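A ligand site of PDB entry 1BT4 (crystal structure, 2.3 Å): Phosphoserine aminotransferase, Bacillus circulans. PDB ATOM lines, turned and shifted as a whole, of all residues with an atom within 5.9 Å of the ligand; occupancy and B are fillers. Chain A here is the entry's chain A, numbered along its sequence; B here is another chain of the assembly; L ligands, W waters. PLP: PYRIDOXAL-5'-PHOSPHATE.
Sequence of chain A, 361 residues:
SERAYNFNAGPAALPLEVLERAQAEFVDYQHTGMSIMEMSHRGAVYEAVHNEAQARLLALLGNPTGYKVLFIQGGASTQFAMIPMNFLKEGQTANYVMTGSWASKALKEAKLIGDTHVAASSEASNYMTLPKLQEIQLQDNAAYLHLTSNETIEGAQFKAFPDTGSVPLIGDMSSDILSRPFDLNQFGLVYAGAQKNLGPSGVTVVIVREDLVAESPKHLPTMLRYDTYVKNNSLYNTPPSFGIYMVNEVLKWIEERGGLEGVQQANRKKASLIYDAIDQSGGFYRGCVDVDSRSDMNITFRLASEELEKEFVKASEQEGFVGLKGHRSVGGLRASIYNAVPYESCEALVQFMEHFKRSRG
OG of Ser 174 lies within hydrogen-bond range of OD1 of Asp 172 (2.8 Å). The side-chain hydroxyl of Thr 152 lies within hydrogen-bond range of the side-chain hydroxyl of Ser 175. O of Thr 238 of chain B sits at hydrogen-bond distance from NE2 of Gln 73 of chain B, at 3.5 Å. The side-chain amide nitrogen of Asn 237 of chain B sits at hydrogen-bond distance from the backbone carbonyl oxygen of Gly 74, 3.2 Å away. The side-chain hydroxyl (OG) of Ser 174 sits at hydrogen-bond distance from the backbone NH (N) of Gly 193, 3.3 Å away. OG1 of Thr 204 sits close to N of Gly 75 (3.0 Å). N of Trp 102 lies within hydrogen-bond range of OE1 of Glu 151. The side-chain amide nitrogen of Asn 150 lies within hydrogen-bond range of the side-chain hydroxyl of Ser 175 (2.6 Å).
CA of Gly 75 touches O1P of the ligand, 3.3 Å away. Phe 80 touches the ligand (CZ to C6, 3.7 Å). CE3 of Trp 102 touches C6 of the ligand, at 3.5 Å. Thr 148 touches the ligand. Asn 150 touches the ligand (O to C2A, 3.8 Å). Ser 174 touches the ligand. Ser 175 touches the ligand. Within 4 Å of the ligand: Gly 75, Ala 76, Ser 77, Phe 80, Trp 102, Thr 148, Asn 150, Thr 152, Asp 172, Ser 174, Ser 175, Gln 195, Lys 196, Asn 237 of chain B and Thr 238 of chain B.
Water W1 lies within hydrogen-bond range of O of Thr 238 of chain B (2.6 Å), O1P of the ligand (2.8 Å) and NE2 of Gln 73 of chain B (3.2 Å). Water W2 lies within hydrogen-bond range of the backbone carbonyl oxygen of Asn 150 (2.6 Å), the backbone carbonyl oxygen of Asp 172 (3.1 Å) and the side-chain hydroxyl of Ser 175 (3.2 Å).
NZ of Lys 196 is bonded to C4A of the ligand, 1.5 Å away. N1 of the ligand sits at hydrogen-bond distance from OD2 of Asp 172, 2.7 Å away. An oxygen (O3) of the ligand sits at hydrogen-bond distance from the side-chain hydroxyl of Thr 152. The side-chain amide nitrogen (NE2) of Gln 195 is in hydrogen-bond range of an oxygen (O1P) of the ligand. N of Ser 77 is in hydrogen-bond range of O3P of the ligand (3.0 Å). The side-chain hydroxyl (OG) of Ser 77 lies within hydrogen-bond range of an oxygen (O3P) of the ligand, 2.7 Å away. N of Thr 238 of chain B is in hydrogen-bond range of O2P of the ligand, 3.0 Å away. An oxygen (O2P) of the ligand lies within hydrogen-bond range of the side-chain hydroxyl (OG1) of Thr 238 of chain B (2.8 Å). The side-chain amide nitrogen (ND2) of Asn 237 of chain B sits at hydrogen-bond distance from an oxygen (O3P) of the ligand, 3.1 Å away. An oxygen (O3P) of the ligand lies within hydrogen-bond range of the backbone NH of Ala 76, 3.3 Å away.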
ATOM      1  N   GLY A  74     -25.430 -15.038   6.178  1.00  0.00           N
ATOM      2  CA  GLY A  74     -24.180 -14.761   5.494  1.00  0.00           C
ATOM      3  C   GLY A  74     -23.235 -13.751   6.135  1.00  0.00           C
ATOM      4  O   GLY A  74     -22.114 -13.584   5.661  1.00  0.00           O
ATOM      5  N   GLY A  75     -23.678 -13.070   7.187  1.00  0.00           N
ATOM      6  CA  GLY A  75     -22.824 -12.099   7.841  1.00  0.00           C
ATOM      7  C   GLY A  75     -22.708 -10.798   7.070  1.00  0.00           C
ATOM      8  O   GLY A  75     -23.261 -10.670   5.970  1.00  0.00           O
ATOM      9  N   ALA A  76     -22.034  -9.822   7.668  1.00  0.00           N
ATOM     10  CA  ALA A  76     -21.831  -8.548   7.013  1.00  0.00           C
ATOM     11  C   ALA A  76     -20.979  -8.724   5.760  1.00  0.00           C
ATOM     12  O   ALA A  76     -21.046  -7.908   4.843  1.00  0.00           O
ATOM     13  CB  ALA A  76     -21.160  -7.564   7.980  1.00  0.00           C
ATOM     14  N   SER A  77     -20.207  -9.809   5.716  1.00  0.00           N
ATOM     15  CA  SER A  77     -19.344 -10.097   4.563  1.00  0.00           C
ATOM     16  C   SER A  77     -20.153 -10.342   3.287  1.00  0.00           C
ATOM     17  O   SER A  77     -19.780  -9.880   2.228  1.00  0.00           O
ATOM     18  CB  SER A  77     -18.462 -11.323   4.844  1.00  0.00           C
ATOM     19  OG  SER A  77     -17.484 -11.042   5.827  1.00  0.00           O
ATOM     20  N   THR A  78     -21.237 -11.112   3.391  1.00  0.00           N
ATOM     21  CA  THR A  78     -22.046 -11.391   2.211  1.00  0.00           C
ATOM     22  C   THR A  78     -22.657 -10.101   1.687  1.00  0.00           C
ATOM     23  O   THR A  78     -22.875  -9.952   0.482  1.00  0.00           O
ATOM     24  CB  THR A  78     -23.118 -12.455   2.529  1.00  0.00           C
ATOM     25  OG1 THR A  78     -22.471 -13.715   2.763  1.00  0.00           O
ATOM     26  CG2 THR A  78     -24.134 -12.599   1.372  1.00  0.00           C
ATOM     27  N   PHE A  80     -21.157  -7.372   1.561  1.00  0.00           N
ATOM     28  CA  PHE A  80     -20.087  -6.711   0.798  1.00  0.00           C
ATOM     29  C   PHE A  80     -20.297  -6.951  -0.700  1.00  0.00           C
ATOM     30  O   PHE A  80     -20.013  -6.078  -1.520  1.00  0.00           O
ATOM     31  CB  PHE A  80     -18.716  -7.233   1.225  1.00  0.00           C
ATOM     32  CG  PHE A  80     -18.253  -6.746   2.584  1.00  0.00           C
ATOM     33  CD1 PHE A  80     -19.004  -5.803   3.300  1.00  0.00           C
ATOM     34  CD2 PHE A  80     -17.067  -7.200   3.126  1.00  0.00           C
ATOM     35  CE1 PHE A  80     -18.565  -5.333   4.545  1.00  0.00           C
ATOM     36  CE2 PHE A  80     -16.621  -6.737   4.370  1.00  0.00           C
ATOM     37  CZ  PHE A  80     -17.365  -5.800   5.076  1.00  0.00           C
ATOM     38  N   TRP A 102     -12.015  -2.934   7.380  1.00  0.00           N
ATOM     39  CA  TRP A 102     -13.341  -3.362   6.929  1.00  0.00           C
ATOM     40  C   TRP A 102     -13.819  -2.578   5.732  1.00  0.00           C
ATOM     41  O   TRP A 102     -14.509  -3.125   4.868  1.00  0.00           O
ATOM     42  CB  TRP A 102     -14.347  -3.352   8.079  1.00  0.00           C
ATOM     43  CG  TRP A 102     -14.151  -4.515   8.979  1.00  0.00           C
ATOM     44  CD1 TRP A 102     -13.807  -4.481  10.297  1.00  0.00           C
ATOM     45  CD2 TRP A 102     -14.226  -5.898   8.615  1.00  0.00           C
ATOM     46  NE1 TRP A 102     -13.670  -5.761  10.779  1.00  0.00           N
ATOM     47  CE2 TRP A 102     -13.916  -6.646   9.766  1.00  0.00           C
ATOM     48  CE3 TRP A 102     -14.524  -6.581   7.421  1.00  0.00           C
ATOM     49  CZ2 TRP A 102     -13.904  -8.045   9.773  1.00  0.00           C
ATOM     50  CZ3 TRP A 102     -14.507  -7.965   7.422  1.00  0.00           C
ATOM     51  CH2 TRP A 102     -14.207  -8.685   8.588  1.00  0.00           C
ATOM     52  N   THR A 148     -17.904   2.823   6.570  1.00  0.00           N
ATOM     53  CA  THR A 148     -17.846   1.940   7.731  1.00  0.00           C
ATOM     54  C   THR A 148     -17.966   2.899   8.906  1.00  0.00           C
ATOM     55  O   THR A 148     -17.077   3.710   9.130  1.00  0.00           O
ATOM     56  CB  THR A 148     -16.483   1.197   7.787  1.00  0.00           C
ATOM     57  OG1 THR A 148     -16.320   0.439   6.585  1.00  0.00           O
ATOM     58  CG2 THR A 148     -16.430   0.237   8.959  1.00  0.00           C
ATOM     59  N   ASN A 150     -17.940   2.295  12.165  1.00  0.00           N
ATOM     60  CA  ASN A 150     -16.963   1.963  13.209  1.00  0.00           C
ATOM     61  C   ASN A 150     -15.982   0.926  12.674  1.00  0.00           C
ATOM     62  O   ASN A 150     -16.398  -0.145  12.221  1.00  0.00           O
ATOM     63  CB  ASN A 150     -17.660   1.406  14.472  1.00  0.00           C
ATOM     64  CG  ASN A 150     -16.702   1.215  15.662  1.00  0.00           C
ATOM     65  OD1 ASN A 150     -16.171   2.173  16.205  1.00  0.00           O
ATOM     66  ND2 ASN A 150     -16.496  -0.035  16.070  1.00  0.00           N
ATOM     67  N   GLU A 151     -14.692   1.280  12.668  1.00  0.00           N
ATOM     68  CA  GLU A 151     -13.636   0.369  12.222  1.00  0.00           C
ATOM     69  C   GLU A 151     -13.186  -0.481  13.408  1.00  0.00           C
ATOM     70  O   GLU A 151     -12.333  -0.081  14.185  1.00  0.00           O
ATOM     71  CB  GLU A 151     -12.447   1.143  11.616  1.00  0.00           C
ATOM     72  CG  GLU A 151     -12.653   1.651  10.186  1.00  0.00           C
ATOM     73  CD  GLU A 151     -12.797   0.536   9.128  1.00  0.00           C
ATOM     74  OE1 GLU A 151     -12.693  -0.664   9.454  1.00  0.00           O
ATOM     75  OE2 GLU A 151     -12.998   0.875   7.952  1.00  0.00           O
ATOM     76  N   THR A 152     -13.791  -1.644  13.535  1.00  0.00           N
ATOM     77  CA  THR A 152     -13.543  -2.584  14.615  1.00  0.00           C
ATOM     78  C   THR A 152     -12.074  -2.903  14.892  1.00  0.00           C
ATOM     79  O   THR A 152     -11.657  -3.009  16.054  1.00  0.00           O
ATOM     80  CB  THR A 152     -14.270  -3.910  14.341  1.00  0.00           C
ATOM     81  OG1 THR A 152     -15.539  -3.630  13.750  1.00  0.00           O
ATOM     82  CG2 THR A 152     -14.493  -4.683  15.639  1.00  0.00           C
ATOM     83  N   ASP A 172     -21.806   0.320   6.930  1.00  0.00           N
ATOM     84  CA  ASP A 172     -21.533  -0.916   7.640  1.00  0.00           C
ATOM     85  C   ASP A 172     -21.481  -0.539   9.128  1.00  0.00           C
ATOM     86  O   ASP A 172     -20.542   0.147   9.573  1.00  0.00           O
ATOM     87  CB  ASP A 172     -20.189  -1.497   7.186  1.00  0.00           C
ATOM     88  CG  ASP A 172     -19.862  -2.813   7.855  1.00  0.00           C
ATOM     89  OD1 ASP A 172     -20.547  -3.221   8.822  1.00  0.00           O
ATOM     90  OD2 ASP A 172     -18.896  -3.454   7.382  1.00  0.00           O
ATOM     91  N   MET A 173     -22.510  -0.940   9.868  1.00  0.00           N
ATOM     92  CA  MET A 173     -22.581  -0.628  11.295  1.00  0.00           C
ATOM     93  C   MET A 173     -22.487  -1.869  12.165  1.00  0.00           C
ATOM     94  O   MET A 173     -22.987  -1.878  13.289  1.00  0.00           O
ATOM     95  CB  MET A 173     -23.875   0.122  11.622  1.00  0.00           C
ATOM     96  CG  MET A 173     -23.941   1.531  11.060  1.00  0.00           C
ATOM     97  SD  MET A 173     -25.459   2.380  11.523  1.00  0.00           S
ATOM     98  CE  MET A 173     -25.127   4.071  10.976  1.00  0.00           C
ATOM     99  N   SER A 174     -21.807  -2.894  11.655  1.00  0.00           N
ATOM    100  CA  SER A 174     -21.649  -4.149  12.378  1.00  0.00           C
ATOM    101  C   SER A 174     -21.231  -3.958  13.834  1.00  0.00           C
ATOM    102  O   SER A 174     -21.900  -4.470  14.736  1.00  0.00           O
ATOM    103  CB  SER A 174     -20.645  -5.058  11.690  1.00  0.00           C
ATOM    104  OG  SER A 174     -21.081  -5.447  10.393  1.00  0.00           O
ATOM    105  N   SER A 175     -20.204  -3.152  14.063  1.00  0.00           N
ATOM    106  CA  SER A 175     -19.710  -2.947  15.422  1.00  0.00           C
ATOM    107  C   SER A 175     -20.249  -1.789  16.267  1.00  0.00           C
ATOM    108  O   SER A 175     -19.849  -1.651  17.422  1.00  0.00           O
ATOM    109  CB  SER A 175     -18.173  -3.000  15.452  1.00  0.00           C
ATOM    110  OG  SER A 175     -17.609  -1.944  14.703  1.00  0.00           O
ATOM    111  N   TYR A 191     -26.436  -1.765   7.495  1.00  0.00           N
ATOM    112  CA  TYR A 191     -26.348  -3.202   7.771  1.00  0.00           C
ATOM    113  C   TYR A 191     -25.418  -3.540   8.919  1.00  0.00           C
ATOM    114  O   TYR A 191     -24.538  -2.760   9.258  1.00  0.00           O
ATOM    115  CB  TYR A 191     -25.987  -4.000   6.505  1.00  0.00           C
ATOM    116  CG  TYR A 191     -24.606  -3.743   5.939  1.00  0.00           C
ATOM    117  CD1 TYR A 191     -24.317  -2.575   5.234  1.00  0.00           C
ATOM    118  CD2 TYR A 191     -23.602  -4.711   6.045  1.00  0.00           C
ATOM    119  CE1 TYR A 191     -23.077  -2.376   4.645  1.00  0.00           C
ATOM    120  CE2 TYR A 191     -22.357  -4.520   5.455  1.00  0.00           C
ATOM    121  CZ  TYR A 191     -22.107  -3.356   4.762  1.00  0.00           C
ATOM    122  OH  TYR A 191     -20.892  -3.183   4.152  1.00  0.00           O
ATOM    123  N   GLY A 193     -23.777  -7.282  11.143  1.00  0.00           N
ATOM    124  CA  GLY A 193     -23.772  -8.670  11.561  1.00  0.00           C
ATOM    125  C   GLY A 193     -24.229  -8.526  13.014  1.00  0.00           C
ATOM    126  O   GLY A 193     -23.783  -7.617  13.706  1.00  0.00           O
ATOM    127  N   GLN A 195     -23.755 -10.533  15.665  1.00  0.00           N
ATOM    128  CA  GLN A 195     -22.805 -11.012  16.667  1.00  0.00           C
ATOM    129  C   GLN A 195     -21.898 -10.009  17.361  1.00  0.00           C
ATOM    130  O   GLN A 195     -21.257 -10.334  18.358  1.00  0.00           O
ATOM    131  CB  GLN A 195     -21.928 -12.116  16.094  1.00  0.00           C
ATOM    132  CG  GLN A 195     -20.875 -11.660  15.088  1.00  0.00           C
ATOM    133  CD  GLN A 195     -21.436 -11.444  13.683  1.00  0.00           C
ATOM    134  OE1 GLN A 195     -22.645 -11.572  13.445  1.00  0.00           O
ATOM    135  NE2 GLN A 195     -20.550 -11.132  12.744  1.00  0.00           N
ATOM    136  N   LYS A 196     -21.816  -8.805  16.822  1.00  0.00           N
ATOM    137  CA  LYS A 196     -20.962  -7.803  17.421  1.00  0.00           C
ATOM    138  C   LYS A 196     -21.623  -7.025  18.556  1.00  0.00           C
ATOM    139  O   LYS A 196     -21.105  -6.973  19.673  1.00  0.00           O
ATOM    140  CB  LYS A 196     -20.479  -6.851  16.325  1.00  0.00           C
ATOM    141  CG  LYS A 196     -19.063  -7.086  15.813  1.00  0.00           C
ATOM    142  CD  LYS A 196     -18.736  -8.440  15.108  1.00  0.00           C
ATOM    143  CE  LYS A 196     -17.288  -8.229  14.712  1.00  0.00           C
ATOM    144  NZ  LYS A 196     -17.170  -7.434  13.461  1.00  0.00           N
ATOM    145  N   THR A 204     -27.821 -11.297   9.971  1.00  0.00           N
ATOM    146  CA  THR A 204     -27.385  -9.965   9.567  1.00  0.00           C
ATOM    147  C   THR A 204     -28.647  -9.120   9.431  1.00  0.00           C
ATOM    148  O   THR A 204     -29.618  -9.515   8.767  1.00  0.00           O
ATOM    149  CB  THR A 204     -26.649  -9.977   8.204  1.00  0.00           C
ATOM    150  OG1 THR A 204     -25.623 -10.969   8.225  1.00  0.00           O
ATOM    151  CG2 THR A 204     -25.994  -8.630   7.923  1.00  0.00           C
ATOM    152  N   TYR A 338     -18.681  -3.269  23.848  1.00  0.00           N
ATOM    153  CA  TYR A 338     -20.023  -3.162  23.284  1.00  0.00           C
ATOM    154  C   TYR A 338     -21.107  -2.956  24.371  1.00  0.00           C
ATOM    155  O   TYR A 338     -20.815  -3.041  25.565  1.00  0.00           O
ATOM    156  CB  TYR A 338     -20.335  -4.429  22.479  1.00  0.00           C
ATOM    157  CG  TYR A 338     -19.346  -4.710  21.375  1.00  0.00           C
ATOM    158  CD1 TYR A 338     -19.115  -3.768  20.372  1.00  0.00           C
ATOM    159  CD2 TYR A 338     -18.661  -5.925  21.323  1.00  0.00           C
ATOM    160  CE1 TYR A 338     -18.210  -4.016  19.342  1.00  0.00           C
ATOM    161  CE2 TYR A 338     -17.754  -6.196  20.289  1.00  0.00           C
ATOM    162  CZ  TYR A 338     -17.535  -5.228  19.311  1.00  0.00           C
ATOM    163  OH  TYR A 338     -16.646  -5.476  18.289  1.00  0.00           O
ATOM    164  N   GLN B  73     -23.749 -20.564   5.549  1.00  0.00           N
ATOM    165  CA  GLN B  73     -25.033 -19.925   5.841  1.00  0.00           C
ATOM    166  C   GLN B  73     -25.889 -19.815   4.579  1.00  0.00           C
ATOM    167  O   GLN B  73     -25.417 -20.118   3.468  1.00  0.00           O
ATOM    168  CB  GLN B  73     -24.801 -18.533   6.439  1.00  0.00           C
ATOM    169  CG  GLN B  73     -24.120 -18.541   7.795  1.00  0.00           C
ATOM    170  CD  GLN B  73     -24.001 -17.154   8.410  1.00  0.00           C
ATOM    171  OE1 GLN B  73     -25.001 -16.502   8.679  1.00  0.00           O
ATOM    172  NE2 GLN B  73     -22.773 -16.706   8.614  1.00  0.00           N
ATOM    173  N   TYR B 236     -13.583 -18.157   7.534  1.00  0.00           N
ATOM    174  CA  TYR B 236     -13.218 -16.914   6.832  1.00  0.00           C
ATOM    175  C   TYR B 236     -13.918 -15.697   7.469  1.00  0.00           C
ATOM    176  O   TYR B 236     -13.326 -14.632   7.620  1.00  0.00           O
ATOM    177  CB  TYR B 236     -13.625 -17.010   5.349  1.00  0.00           C
ATOM    178  CG  TYR B 236     -13.372 -15.730   4.612  1.00  0.00           C
ATOM    179  CD1 TYR B 236     -12.064 -15.301   4.356  1.00  0.00           C
ATOM    180  CD2 TYR B 236     -14.428 -14.900   4.210  1.00  0.00           C
ATOM    181  CE1 TYR B 236     -11.806 -14.089   3.729  1.00  0.00           C
ATOM    182  CE2 TYR B 236     -14.179 -13.669   3.575  1.00  0.00           C
ATOM    183  CZ  TYR B 236     -12.858 -13.270   3.335  1.00  0.00           C
ATOM    184  OH  TYR B 236     -12.583 -12.072   2.719  1.00  0.00           O
ATOM    185  N   ASN B 237     -15.208 -15.863   7.761  1.00  0.00           N
ATOM    186  CA  ASN B 237     -15.972 -14.814   8.428  1.00  0.00           C
ATOM    187  C   ASN B 237     -16.639 -15.513   9.621  1.00  0.00           C
ATOM    188  O   ASN B 237     -16.512 -16.739   9.756  1.00  0.00           O
ATOM    189  CB  ASN B 237     -16.987 -14.165   7.475  1.00  0.00           C
ATOM    190  CG  ASN B 237     -18.238 -14.994   7.288  1.00  0.00           C
ATOM    191  OD1 ASN B 237     -18.185 -16.226   7.229  1.00  0.00           O
ATOM    192  ND2 ASN B 237     -19.377 -14.315   7.210  1.00  0.00           N
ATOM    193  N   THR B 238     -17.312 -14.764  10.495  1.00  0.00           N
ATOM    194  CA  THR B 238     -17.971 -15.346  11.666  1.00  0.00           C
ATOM    195  C   THR B 238     -18.977 -16.425  11.279  1.00  0.00           C
ATOM    196  O   THR B 238     -19.938 -16.164  10.558  1.00  0.00           O
ATOM    197  CB  THR B 238     -18.688 -14.281  12.482  1.00  0.00           C
ATOM    198  OG1 THR B 238     -17.846 -13.125  12.571  1.00  0.00           O
ATOM    199  CG2 THR B 238     -18.962 -14.795  13.875  1.00  0.00           C
HETATM  200  N1  PLP L   1     -17.661  -5.250   8.897  1.00  0.00           N
HETATM  201  C2  PLP L   1     -17.498  -4.738  10.148  1.00  0.00           C
HETATM  202  C2A PLP L   1     -17.379  -3.255  10.315  1.00  0.00           C
HETATM  203  C3  PLP L   1     -17.459  -5.636  11.217  1.00  0.00           C
HETATM  204  O3  PLP L   1     -17.273  -5.180  12.469  1.00  0.00           O
HETATM  205  C4  PLP L   1     -17.589  -7.011  10.990  1.00  0.00           C
HETATM  206  C4A PLP L   1     -17.664  -7.939  12.186  1.00  0.00           C
HETATM  207  C5  PLP L   1     -17.738  -7.492   9.646  1.00  0.00           C
HETATM  208  C6  PLP L   1     -17.774  -6.573   8.635  1.00  0.00           C
HETATM  209  C5A PLP L   1     -17.789  -8.978   9.261  1.00  0.00           C
HETATM  210  O4P PLP L   1     -18.916  -9.612   9.861  1.00  0.00           O
HETATM  211  P   PLP L   1     -19.096 -11.193   9.553  1.00  0.00           P
HETATM  212  O1P PLP L   1     -20.450 -11.574  10.095  1.00  0.00           O
HETATM  213  O2P PLP L   1     -17.882 -11.882  10.096  1.00  0.00           O
HETATM  214  O3P PLP L   1     -19.113 -11.332   7.994  1.00  0.00           O
HETATM  215  O   HOH W   1     -21.463 -14.167  10.103  1.00  0.00           O
HETATM  216  O   HOH W   2     -18.909  -0.795  12.008  1.00  0.00           O
HETATM  217  O   HOH W   3     -15.305 -11.476   9.937  1.00  0.00           O
HETATM  218  O   HOH W   4     -15.182 -10.142  12.588  1.00  0.00           O
